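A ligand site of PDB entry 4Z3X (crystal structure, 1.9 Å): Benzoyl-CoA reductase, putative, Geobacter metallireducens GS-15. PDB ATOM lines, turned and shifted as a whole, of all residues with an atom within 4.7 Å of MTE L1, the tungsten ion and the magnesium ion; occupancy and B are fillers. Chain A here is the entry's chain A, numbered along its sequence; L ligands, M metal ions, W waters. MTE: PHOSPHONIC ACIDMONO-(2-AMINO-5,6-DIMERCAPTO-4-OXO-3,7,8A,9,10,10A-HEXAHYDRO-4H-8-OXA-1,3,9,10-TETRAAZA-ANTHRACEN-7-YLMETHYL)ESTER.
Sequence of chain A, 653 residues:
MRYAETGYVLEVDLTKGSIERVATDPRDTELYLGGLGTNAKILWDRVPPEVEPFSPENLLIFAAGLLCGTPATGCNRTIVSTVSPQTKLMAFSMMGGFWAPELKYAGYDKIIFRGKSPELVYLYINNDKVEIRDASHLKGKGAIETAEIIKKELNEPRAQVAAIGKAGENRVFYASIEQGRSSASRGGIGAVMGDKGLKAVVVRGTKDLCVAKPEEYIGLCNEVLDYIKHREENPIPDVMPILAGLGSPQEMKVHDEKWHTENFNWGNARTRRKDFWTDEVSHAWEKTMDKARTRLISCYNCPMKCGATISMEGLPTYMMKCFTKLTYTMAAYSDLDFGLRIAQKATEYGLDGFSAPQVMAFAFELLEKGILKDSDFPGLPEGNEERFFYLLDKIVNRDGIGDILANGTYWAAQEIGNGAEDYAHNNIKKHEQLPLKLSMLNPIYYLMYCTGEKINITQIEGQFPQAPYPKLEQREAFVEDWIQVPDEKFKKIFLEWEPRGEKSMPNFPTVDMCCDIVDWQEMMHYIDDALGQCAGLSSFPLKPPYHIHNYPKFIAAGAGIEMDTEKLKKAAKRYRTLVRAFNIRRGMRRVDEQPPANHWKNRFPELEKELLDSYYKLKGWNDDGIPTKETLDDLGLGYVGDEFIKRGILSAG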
ATOM      1  N   ARG A  77      11.514  -3.122 -15.072  1.00  0.00           N
ATOM      2  CA  ARG A  77      10.847  -3.732 -16.230  1.00  0.00           C
ATOM      3  C   ARG A  77      10.107  -2.722 -17.094  1.00  0.00           C
ATOM      4  O   ARG A  77       9.475  -1.794 -16.608  1.00  0.00           O
ATOM      5  CB  ARG A  77       9.855  -4.859 -15.812  1.00  0.00           C
ATOM      6  CG  ARG A  77      10.382  -6.258 -16.162  1.00  0.00           C
ATOM      7  CD  ARG A  77      11.591  -6.721 -15.255  1.00  0.00           C
ATOM      8  NE  ARG A  77      12.152  -7.942 -15.838  1.00  0.00           N
ATOM      9  CZ  ARG A  77      13.352  -8.471 -15.600  1.00  0.00           C
ATOM     10  NH1 ARG A  77      14.250  -7.882 -14.777  1.00  0.00           N
ATOM     11  NH2 ARG A  77      13.677  -9.593 -16.245  1.00  0.00           N
ATOM     12  N   MET A  94       6.807  -8.294 -21.100  1.00  0.00           N
ATOM     13  CA  MET A  94       7.708  -7.647 -20.164  1.00  0.00           C
ATOM     14  C   MET A  94       9.147  -7.788 -20.628  1.00  0.00           C
ATOM     15  O   MET A  94       9.536  -8.824 -21.194  1.00  0.00           O
ATOM     16  CB  MET A  94       7.561  -8.196 -18.743  1.00  0.00           C
ATOM     17  CG  MET A  94       6.604  -7.370 -17.886  1.00  0.00           C
ATOM     18  SD  MET A  94       4.841  -7.650 -18.415  1.00  0.00           S
ATOM     19  CE  MET A  94       4.770  -9.414 -18.445  1.00  0.00           C
ATOM     20  N   MET A  95       9.917  -6.727 -20.413  1.00  0.00           N
ATOM     21  CA  MET A  95      11.350  -6.668 -20.756  1.00  0.00           C
ATOM     22  C   MET A  95      12.179  -6.087 -19.592  1.00  0.00           C
ATOM     23  O   MET A  95      11.851  -5.013 -19.037  1.00  0.00           O
ATOM     24  CB  MET A  95      11.481  -5.814 -22.052  1.00  0.00           C
ATOM     25  CG  MET A  95      12.853  -5.680 -22.619  1.00  0.00           C
ATOM     26  SD  MET A  95      12.902  -4.371 -23.848  1.00  0.00           S
ATOM     27  CE  MET A  95      12.496  -5.268 -25.332  1.00  0.00           C
ATOM     28  N   GLY A  96      13.195  -6.822 -19.144  1.00  0.00           N
ATOM     29  CA  GLY A  96      14.055  -6.367 -18.073  1.00  0.00           C
ATOM     30  C   GLY A  96      15.205  -5.471 -18.559  1.00  0.00           C
ATOM     31  O   GLY A  96      15.043  -4.681 -19.465  1.00  0.00           O
ATOM     32  N   GLY A  97      16.368  -5.586 -17.931  1.00  0.00           N
ATOM     33  CA  GLY A  97      17.542  -4.814 -18.372  1.00  0.00           C
ATOM     34  C   GLY A  97      17.568  -3.395 -17.848  1.00  0.00           C
ATOM     35  O   GLY A  97      17.440  -3.147 -16.620  1.00  0.00           O
ATOM     36  N   ARG A 181      20.475  -7.843 -22.739  1.00  0.00           N
ATOM     37  CA  ARG A 181      20.162  -9.198 -22.231  1.00  0.00           C
ATOM     38  C   ARG A 181      18.642  -9.345 -21.883  1.00  0.00           C
ATOM     39  O   ARG A 181      18.254 -10.146 -20.994  1.00  0.00           O
ATOM     40  CB  ARG A 181      21.001  -9.560 -20.973  1.00  0.00           C
ATOM     41  CG  ARG A 181      20.762  -8.644 -19.754  1.00  0.00           C
ATOM     42  CD  ARG A 181      20.855  -9.440 -18.460  1.00  0.00           C
ATOM     43  NE  ARG A 181      19.590 -10.208 -18.325  1.00  0.00           N
ATOM     44  CZ  ARG A 181      19.195 -10.846 -17.230  1.00  0.00           C
ATOM     45  NH1 ARG A 181      19.980 -10.875 -16.157  1.00  0.00           N
ATOM     46  NH2 ARG A 181      18.018 -11.507 -17.247  1.00  0.00           N
ATOM     47  N   SER A 182      17.807  -8.577 -22.588  1.00  0.00           N
ATOM     48  CA  SER A 182      16.400  -8.501 -22.278  1.00  0.00           C
ATOM     49  C   SER A 182      15.524  -8.566 -23.528  1.00  0.00           C
ATOM     50  O   SER A 182      15.942  -8.147 -24.623  1.00  0.00           O
ATOM     51  CB  SER A 182      16.127  -7.224 -21.466  1.00  0.00           C
ATOM     52  OG  SER A 182      17.080  -7.161 -20.393  1.00  0.00           O
ATOM     53  N   SER A 183      14.315  -9.138 -23.367  1.00  0.00           N
ATOM     54  CA  SER A 183      13.405  -9.356 -24.465  1.00  0.00           C
ATOM     55  C   SER A 183      11.905  -9.257 -24.053  1.00  0.00           C
ATOM     56  O   SER A 183      11.535  -9.866 -23.062  1.00  0.00           O
ATOM     57  CB  SER A 183      13.685 -10.726 -25.072  1.00  0.00           C
ATOM     58  OG  SER A 183      12.815 -10.965 -26.182  1.00  0.00           O
ATOM     59  N   ALA A 184      11.147  -8.363 -24.738  1.00  0.00           N
ATOM     60  CA  ALA A 184       9.689  -8.414 -24.789  1.00  0.00           C
ATOM     61  C   ALA A 184       9.417  -9.454 -25.843  1.00  0.00           C
ATOM     62  O   ALA A 184       9.500  -9.191 -27.045  1.00  0.00           O
ATOM     63  CB  ALA A 184       9.049  -7.070 -25.176  1.00  0.00           C
ATOM     64  N   SER A 185       9.155 -10.669 -25.390  1.00  0.00           N
ATOM     65  CA  SER A 185       9.236 -11.810 -26.266  1.00  0.00           C
ATOM     66  C   SER A 185       7.963 -12.239 -27.004  1.00  0.00           C
ATOM     67  O   SER A 185       8.027 -12.619 -28.163  1.00  0.00           O
ATOM     68  CB  SER A 185       9.676 -13.005 -25.437  1.00  0.00           C
ATOM     69  OG  SER A 185      10.835 -12.663 -24.767  1.00  0.00           O
ATOM     70  N   SER A 248      15.010 -15.118 -11.903  1.00  0.00           N
ATOM     71  CA  SER A 248      14.450 -15.973 -12.967  1.00  0.00           C
ATOM     72  C   SER A 248      15.069 -17.363 -12.837  1.00  0.00           C
ATOM     73  O   SER A 248      16.100 -17.489 -12.180  1.00  0.00           O
ATOM     74  CB  SER A 248      14.729 -15.387 -14.348  1.00  0.00           C
ATOM     75  OG  SER A 248      14.272 -14.024 -14.472  1.00  0.00           O
ATOM     76  N   PRO A 249      14.466 -18.416 -13.445  1.00  0.00           N
ATOM     77  CA  PRO A 249      15.111 -19.751 -13.350  1.00  0.00           C
ATOM     78  C   PRO A 249      16.622 -19.701 -13.653  1.00  0.00           C
ATOM     79  O   PRO A 249      17.058 -19.222 -14.715  1.00  0.00           O
ATOM     80  CB  PRO A 249      14.347 -20.550 -14.416  1.00  0.00           C
ATOM     81  CG  PRO A 249      13.021 -20.023 -14.293  1.00  0.00           C
ATOM     82  CD  PRO A 249      13.188 -18.517 -14.146  1.00  0.00           C
ATOM     83  N   LYS A 321      18.882 -15.822 -20.990  1.00  0.00           N
ATOM     84  CA  LYS A 321      18.540 -16.306 -19.641  1.00  0.00           C
ATOM     85  C   LYS A 321      17.389 -17.319 -19.743  1.00  0.00           C
ATOM     86  O   LYS A 321      16.743 -17.439 -20.811  1.00  0.00           O
ATOM     87  CB  LYS A 321      18.130 -15.134 -18.725  1.00  0.00           C
ATOM     88  CG  LYS A 321      16.675 -14.713 -18.828  1.00  0.00           C
ATOM     89  CD  LYS A 321      16.183 -14.335 -20.285  1.00  0.00           C
ATOM     90  CE  LYS A 321      16.762 -12.952 -20.758  1.00  0.00           C
ATOM     91  NZ  LYS A 321      16.169 -12.409 -22.017  1.00  0.00           N
ATOM     92  N   CYS A 322      17.115 -18.052 -18.656  1.00  0.00           N
ATOM     93  CA  CYS A 322      15.946 -18.938 -18.552  1.00  0.00           C
ATOM     94  C   CYS A 322      15.810 -19.964 -19.693  1.00  0.00           C
ATOM     95  O   CYS A 322      16.814 -20.523 -20.197  1.00  0.00           O
ATOM     96  CB  CYS A 322      14.657 -18.085 -18.460  1.00  0.00           C
ATOM     97  SG  CYS A 322      13.204 -18.914 -17.734  1.00  0.00           S
ATOM     98  N   THR A 458       4.403 -19.836 -17.084  1.00  0.00           N
ATOM     99  CA  THR A 458       5.536 -19.450 -16.269  1.00  0.00           C
ATOM    100  C   THR A 458       5.366 -18.007 -15.797  1.00  0.00           C
ATOM    101  O   THR A 458       6.112 -17.522 -14.965  1.00  0.00           O
ATOM    102  CB  THR A 458       6.914 -19.603 -16.980  1.00  0.00           C
ATOM    103  OG1 THR A 458       7.006 -18.685 -18.046  1.00  0.00           O
ATOM    104  CG2 THR A 458       7.107 -20.974 -17.558  1.00  0.00           C
ATOM    105  N   GLN A 459       4.311 -17.353 -16.274  1.00  0.00           N
ATOM    106  CA  GLN A 459       4.102 -15.980 -15.879  1.00  0.00           C
ATOM    107  C   GLN A 459       2.782 -15.762 -15.076  1.00  0.00           C
ATOM    108  O   GLN A 459       2.260 -14.630 -15.001  1.00  0.00           O
ATOM    109  CB  GLN A 459       4.160 -15.098 -17.140  1.00  0.00           C
ATOM    110  CG  GLN A 459       5.608 -14.995 -17.671  1.00  0.00           C
ATOM    111  CD  GLN A 459       5.673 -14.226 -18.941  1.00  0.00           C
ATOM    112  OE1 GLN A 459       5.301 -14.704 -20.008  1.00  0.00           O
ATOM    113  NE2 GLN A 459       6.191 -13.006 -18.840  1.00  0.00           N
ATOM    114  N   ASP A 528       3.605  -6.842  -9.743  1.00  0.00           N
ATOM    115  CA  ASP A 528       4.917  -6.686 -10.360  1.00  0.00           C
ATOM    116  C   ASP A 528       4.875  -5.912 -11.686  1.00  0.00           C
ATOM    117  O   ASP A 528       5.726  -5.021 -11.945  1.00  0.00           O
ATOM    118  CB  ASP A 528       5.561  -8.045 -10.614  1.00  0.00           C
ATOM    119  CG  ASP A 528       5.930  -8.795  -9.332  1.00  0.00           C
ATOM    120  OD1 ASP A 528       5.818  -8.261  -8.177  1.00  0.00           O
ATOM    121  OD2 ASP A 528       6.364  -9.945  -9.511  1.00  0.00           O
ATOM    122  N   ASP A 529       3.941  -6.313 -12.531  1.00  0.00           N
ATOM    123  CA  ASP A 529       3.774  -5.764 -13.861  1.00  0.00           C
ATOM    124  C   ASP A 529       3.234  -4.333 -13.860  1.00  0.00           C
ATOM    125  O   ASP A 529       3.313  -3.638 -14.867  1.00  0.00           O
ATOM    126  CB  ASP A 529       2.864  -6.702 -14.687  1.00  0.00           C
ATOM    127  CG  ASP A 529       3.570  -8.014 -15.018  1.00  0.00           C
ATOM    128  OD1 ASP A 529       4.802  -8.074 -14.774  1.00  0.00           O
ATOM    129  OD2 ASP A 529       2.916  -8.987 -15.462  1.00  0.00           O
ATOM    130  N   GLN A 533       8.521  -4.248 -11.158  1.00  0.00           N
ATOM    131  CA  GLN A 533       9.413  -5.083 -10.324  1.00  0.00           C
ATOM    132  C   GLN A 533       9.736  -6.373 -11.041  1.00  0.00           C
ATOM    133  O   GLN A 533       8.847  -7.012 -11.545  1.00  0.00           O
ATOM    134  CB  GLN A 533       8.778  -5.338  -8.971  1.00  0.00           C
ATOM    135  CG  GLN A 533       9.672  -6.194  -8.025  1.00  0.00           C
ATOM    136  CD  GLN A 533      11.031  -5.538  -7.767  1.00  0.00           C
ATOM    137  OE1 GLN A 533      11.084  -4.412  -7.304  1.00  0.00           O
ATOM    138  NE2 GLN A 533      12.122  -6.231  -8.106  1.00  0.00           N
ATOM    139  N   CYS A 534      10.997  -6.785 -11.094  1.00  0.00           N
ATOM    140  CA  CYS A 534      11.284  -8.122 -11.643  1.00  0.00           C
ATOM    141  C   CYS A 534      10.566  -9.188 -10.807  1.00  0.00           C
ATOM    142  O   CYS A 534      10.764  -9.247  -9.585  1.00  0.00           O
ATOM    143  CB  CYS A 534      12.751  -8.479 -11.647  1.00  0.00           C
ATOM    144  SG  CYS A 534      13.060 -10.026 -12.590  1.00  0.00           S
ATOM    145  N   ALA A 535       9.866 -10.065 -11.491  1.00  0.00           N
ATOM    146  CA  ALA A 535       9.201 -11.221 -10.858  1.00  0.00           C
ATOM    147  C   ALA A 535      10.244 -12.161 -10.189  1.00  0.00           C
ATOM    148  O   ALA A 535       9.888 -12.923  -9.281  1.00  0.00           O
ATOM    149  CB  ALA A 535       8.396 -11.940 -11.870  1.00  0.00           C
ATOM    150  N   GLY A 536      11.502 -12.066 -10.629  1.00  0.00           N
ATOM    151  CA  GLY A 536      12.640 -12.779 -10.014  1.00  0.00           C
ATOM    152  C   GLY A 536      12.875 -12.542  -8.543  1.00  0.00           C
ATOM    153  O   GLY A 536      13.451 -13.393  -7.839  1.00  0.00           O
ATOM    154  N   PHE A 540       7.761 -14.637  -8.756  1.00  0.00           N
ATOM    155  CA  PHE A 540       8.116 -15.932  -9.345  1.00  0.00           C
ATOM    156  C   PHE A 540       8.694 -16.975  -8.337  1.00  0.00           C
ATOM    157  O   PHE A 540       8.188 -18.092  -8.286  1.00  0.00           O
ATOM    158  CB  PHE A 540       9.052 -15.765 -10.511  1.00  0.00           C
ATOM    159  CG  PHE A 540       9.390 -17.081 -11.201  1.00  0.00           C
ATOM    160  CD1 PHE A 540      10.434 -17.886 -10.745  1.00  0.00           C
ATOM    161  CD2 PHE A 540       8.631 -17.506 -12.296  1.00  0.00           C
ATOM    162  CE1 PHE A 540      10.762 -19.079 -11.386  1.00  0.00           C
ATOM    163  CE2 PHE A 540       8.927 -18.714 -12.934  1.00  0.00           C
ATOM    164  CZ  PHE A 540       9.974 -19.511 -12.472  1.00  0.00           C
HETATM  165  N1  MTE L   1       9.284  -9.757 -14.247  1.00  0.00           N
HETATM  166  C2  MTE L   1       8.029  -9.306 -14.441  1.00  0.00           C
HETATM  167  N2  MTE L   1       7.563  -8.125 -13.784  1.00  0.00           N
HETATM  168  N3  MTE L   1       7.058  -9.997 -15.146  1.00  0.00           N
HETATM  169  C4  MTE L   1       7.381 -11.149 -15.819  1.00  0.00           C
HETATM  170  O4  MTE L   1       6.439 -11.750 -16.466  1.00  0.00           O
HETATM  171  N5  MTE L   1       9.158 -12.852 -16.304  1.00  0.00           N
HETATM  172  C6  MTE L   1      10.393 -13.458 -15.653  1.00  0.00           C
HETATM  173  C7  MTE L   1      11.507 -12.456 -15.363  1.00  0.00           C
HETATM  174  N8  MTE L   1      10.963 -11.267 -14.746  1.00  0.00           N
HETATM  175  C9  MTE L   1       8.738 -11.635 -15.666  1.00  0.00           C
HETATM  176  C10 MTE L   1       9.627 -10.911 -14.946  1.00  0.00           C
HETATM  177  C1' MTE L   1      11.173 -14.666 -16.488  1.00  0.00           C
HETATM  178  S1' MTE L   1      10.403 -16.301 -16.365  1.00  0.00           S
HETATM  179  C2' MTE L   1      12.166 -14.438 -17.089  1.00  0.00           C
HETATM  180  S2' MTE L   1      12.881 -15.680 -18.070  1.00  0.00           S
HETATM  181  C3' MTE L   1      12.776 -12.983 -17.241  1.00  0.00           C
HETATM  182  O3' MTE L   1      12.007 -12.013 -16.583  1.00  0.00           O
HETATM  183  C4' MTE L   1      12.732 -12.491 -18.661  1.00  0.00           C
HETATM  184  O4' MTE L   1      13.645 -11.385 -18.819  1.00  0.00           O
HETATM  185  P   MTE L   1      13.441 -10.428 -20.062  1.00  0.00           P
HETATM  186  O1P MTE L   1      13.978 -11.207 -21.336  1.00  0.00           O
HETATM  187  O2P MTE L   1      14.216  -9.120 -19.878  1.00  0.00           O
HETATM  188  O3P MTE L   1      12.061 -10.183 -20.197  1.00  0.00           O
HETATM  189  N1  MTE L   2      12.204 -15.141 -26.394  1.00  0.00           N
HETATM  190  C2  MTE L   2      13.332 -14.489 -26.688  1.00  0.00           C
HETATM  191  N2  MTE L   2      13.560 -14.139 -28.062  1.00  0.00           N
HETATM  192  N3  MTE L   2      14.305 -14.247 -25.705  1.00  0.00           N
HETATM  193  C4  MTE L   2      13.954 -14.666 -24.437  1.00  0.00           C
HETATM  194  O4  MTE L   2      14.756 -14.417 -23.565  1.00  0.00           O
HETATM  195  N5  MTE L   2      12.289 -15.843 -22.865  1.00  0.00           N
HETATM  196  C6  MTE L   2      11.272 -16.955 -22.733  1.00  0.00           C
HETATM  197  C7  MTE L   2      10.128 -16.618 -23.646  1.00  0.00           C
HETATM  198  N8  MTE L   2      10.564 -16.247 -24.946  1.00  0.00           N
HETATM  199  C9  MTE L   2      12.684 -15.410 -24.157  1.00  0.00           C
HETATM  200  C10 MTE L   2      11.835 -15.582 -25.139  1.00  0.00           C
HETATM  201  C1' MTE L   2      10.912 -17.132 -21.241  1.00  0.00           C
HETATM  202  S1' MTE L   2      11.886 -18.183 -20.079  1.00  0.00           S
HETATM  203  C2' MTE L   2       9.928 -16.367 -20.846  1.00  0.00           C
HETATM  204  S2' MTE L   2       9.382 -16.288 -19.233  1.00  0.00           S
HETATM  205  C3' MTE L   2       9.064 -15.493 -21.865  1.00  0.00           C
HETATM  206  O3' MTE L   2       9.604 -15.387 -23.164  1.00  0.00           O
HETATM  207  C4' MTE L   2       8.628 -14.134 -21.320  1.00  0.00           C
HETATM  208  O4' MTE L   2       7.723 -13.457 -22.181  1.00  0.00           O
HETATM  209  P   MTE L   2       7.562 -11.907 -22.339  1.00  0.00           P
HETATM  210  O1P MTE L   2       6.508 -11.600 -23.449  1.00  0.00           O
HETATM  211  O2P MTE L   2       8.936 -11.293 -22.725  1.00  0.00           O
HETATM  212  O3P MTE L   2       6.979 -11.305 -21.049  1.00  0.00           O
HETATM  213  W     W M   1      11.217 -17.472 -18.043  1.00  0.00           W
HETATM  214 MG    MG M   2      10.448 -10.670 -21.481  1.00  0.00          MG
HETATM  215  O   HOH W   1       9.291 -11.366 -19.816  1.00  0.00           O
HETATM  216  O   HOH W   2      11.575 -12.365 -22.284  1.00  0.00           O
HETATM  217  O   HOH W   3       4.135 -11.578 -14.890  1.00  0.00           O
HETATM  218  O   HOH W   4      10.572  -9.638 -17.919  1.00  0.00           O
HETATM  219  O   HOH W   5       7.269 -14.770 -14.525  1.00  0.00           O
HETATM  220  O   HOH W   6      16.492  -9.160 -18.844  1.00  0.00           O
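The magnesium ion is bound by an oxygen (O2P) of MTE L2 (2.1 Å), the backbone carbonyl oxygen (O) of Met 94 (2.1 Å), the backbone carbonyl oxygen (O) of Ser 183 (2.1 Å), an oxygen (O3P) of MTE L1 (2.1 Å), water W1 (2.1 Å) and water W2 (2.2 Å).
The magnesium ion has six donor atoms within binding distance.
Residues that only touch the magnesium ion: Ser 185 (3.9 Å).
Within 4 Å of the magnesium ion: Met 94, Ser 183 and Ser 185.
The nearest printed residue that does not touch the magnesium ion is Ala 184 (4.1 Å).
Within 4 Å of the tungsten ion: Cys 322.
The nearest printed residue that does not touch the tungsten ion is Thr 458 (4.4 Å).
Residues that only touch MTE L1: Met 95 (3.6 Å), Ser 182 (3.1 Å), Ser 248 (3.3 Å) and Asp 528 (3.8 Å).
Hydrophobic or aromatic side chains that line MTE L1: Met 94 and Ala 535.
The nearest printed residue that does not touch MTE L1 is Pro 249 (4.2 Å).
The backbone NH of Ser 183 lies within hydrogen-bond range of an oxygen (O1P) of MTE L1 (2.9 Å).
The side-chain amino group (NZ) of Lys 321 is in salt-bridge range of an oxygen (O1P) of MTE L1 (2.6 Å).
The backbone NH (N) of Gly 96 lies within hydrogen-bond range of an oxygen (O2P) of MTE L1, 2.6 Å away.
The side-chain amide nitrogen of Gln 459 is in hydrogen-bond range of an oxygen (O4) of MTE L1 (2.7 Å).
N2 of MTE L1 sits at hydrogen-bond distance from O of Gln 533 (2.8 Å).
The backbone NH of Ala 535 lies within hydrogen-bond range of a nitrogen (N1) of MTE L1, 2.8 Å away.
The side-chain carboxylate of Asp 529 is in hydrogen-bond range of a nitrogen (N2) of MTE L1, 2.9 Å away.
O2P of MTE L1 is in salt-bridge range of NH2 of Arg 77, 3.7 Å away.
The side-chain sulfur (SG) of Cys 534 lies close to a nitrogen (N8) of MTE L1.
N of Met 94 is in hydrogen-bond range of O3P of MTE L2.
NZ of Lys 321 lies within hydrogen-bond range of O4 of MTE L2 (2.9 Å).
The side-chain amide nitrogen (NE2) of Gln 459 lies within hydrogen-bond range of an oxygen (O3P) of MTE L2 (2.9 Å).
N of Ser 185 lies within hydrogen-bond range of O1P of MTE L2, at 3.4 Å.
A nitrogen (N1) of MTE L2 lies close to the side-chain hydroxyl of Ser 185, 3.3 Å away.
The side-chain hydroxyl (OG1) of Thr 458 lies close to a sulfur (S2') of MTE L2, at 3.6 Å.
Water W2 bridges the side-chain hydroxyl of Ser 185 (2.6 Å) and an oxygen (O1P) of MTE L1 (2.8 Å).
Water W6 lies within hydrogen-bond range of an oxygen (O2P) of MTE L1 (2.5 Å), the side-chain hydroxyl of Ser 182 (2.6 Å) and the backbone carbonyl oxygen of Arg 181 (2.9 Å).
Water W4 lies within hydrogen-bond range of an oxygen (O3') of MTE L1 and the guanidinium group (NE) of Arg 77.
Water W3 lies within hydrogen-bond range of an oxygen (O4) of MTE L1 (2.8 Å) and the side-chain carboxylate of Asp 529 (2.9 Å).
Water W5 lies within hydrogen-bond range of the backbone carbonyl oxygen of Thr 458 (3.0 Å) and a nitrogen (N5) of MTE L1 (3.2 Å).
S1' of MTE L1 is bound to the tungsten ion, 2.2 Å away.
S1' of MTE L2 binds the tungsten ion, 2.3 Å away.
The tungsten ion is bound by S2' of MTE L1, 2.4 Å away.
SG of Cys 322 is bound to the tungsten ion.
A sulfur (S2') of MTE L2 is bound to the tungsten ion (2.5 Å).
The side-chain hydroxyl of Ser 185 is in hydrogen-bond range of the side-chain hydroxyl of Ser 183, at 3.0 Å.
The side-chain amino group (NZ) of Lys 321 sits close to the backbone carbonyl oxygen (O) of Arg 181 (3.2 Å).
The backbone carbonyl oxygen (O) of Gly 96 sits close to the side-chain hydroxyl (OG) of Ser 182, 3.3 Å away.
N of Gln 533 lies within hydrogen-bond range of O of Asp 528.
The backbone carbonyl oxygen (O) of Ala 535 lies within hydrogen-bond range of the backbone NH (N) of Phe 540 (2.8 Å).
The side-chain sulfur of Cys 534 sits close to the guanidinium group of Arg 77 (3.3 Å).
The side-chain hydroxyl (OG) of Ser 182 sits at hydrogen-bond distance from the backbone NH (N) of Gly 97, 3.0 Å away.
The backbone NH (N) of Gly 536 lies close to the side-chain sulfur (SG) of Cys 534 (3.2 Å).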
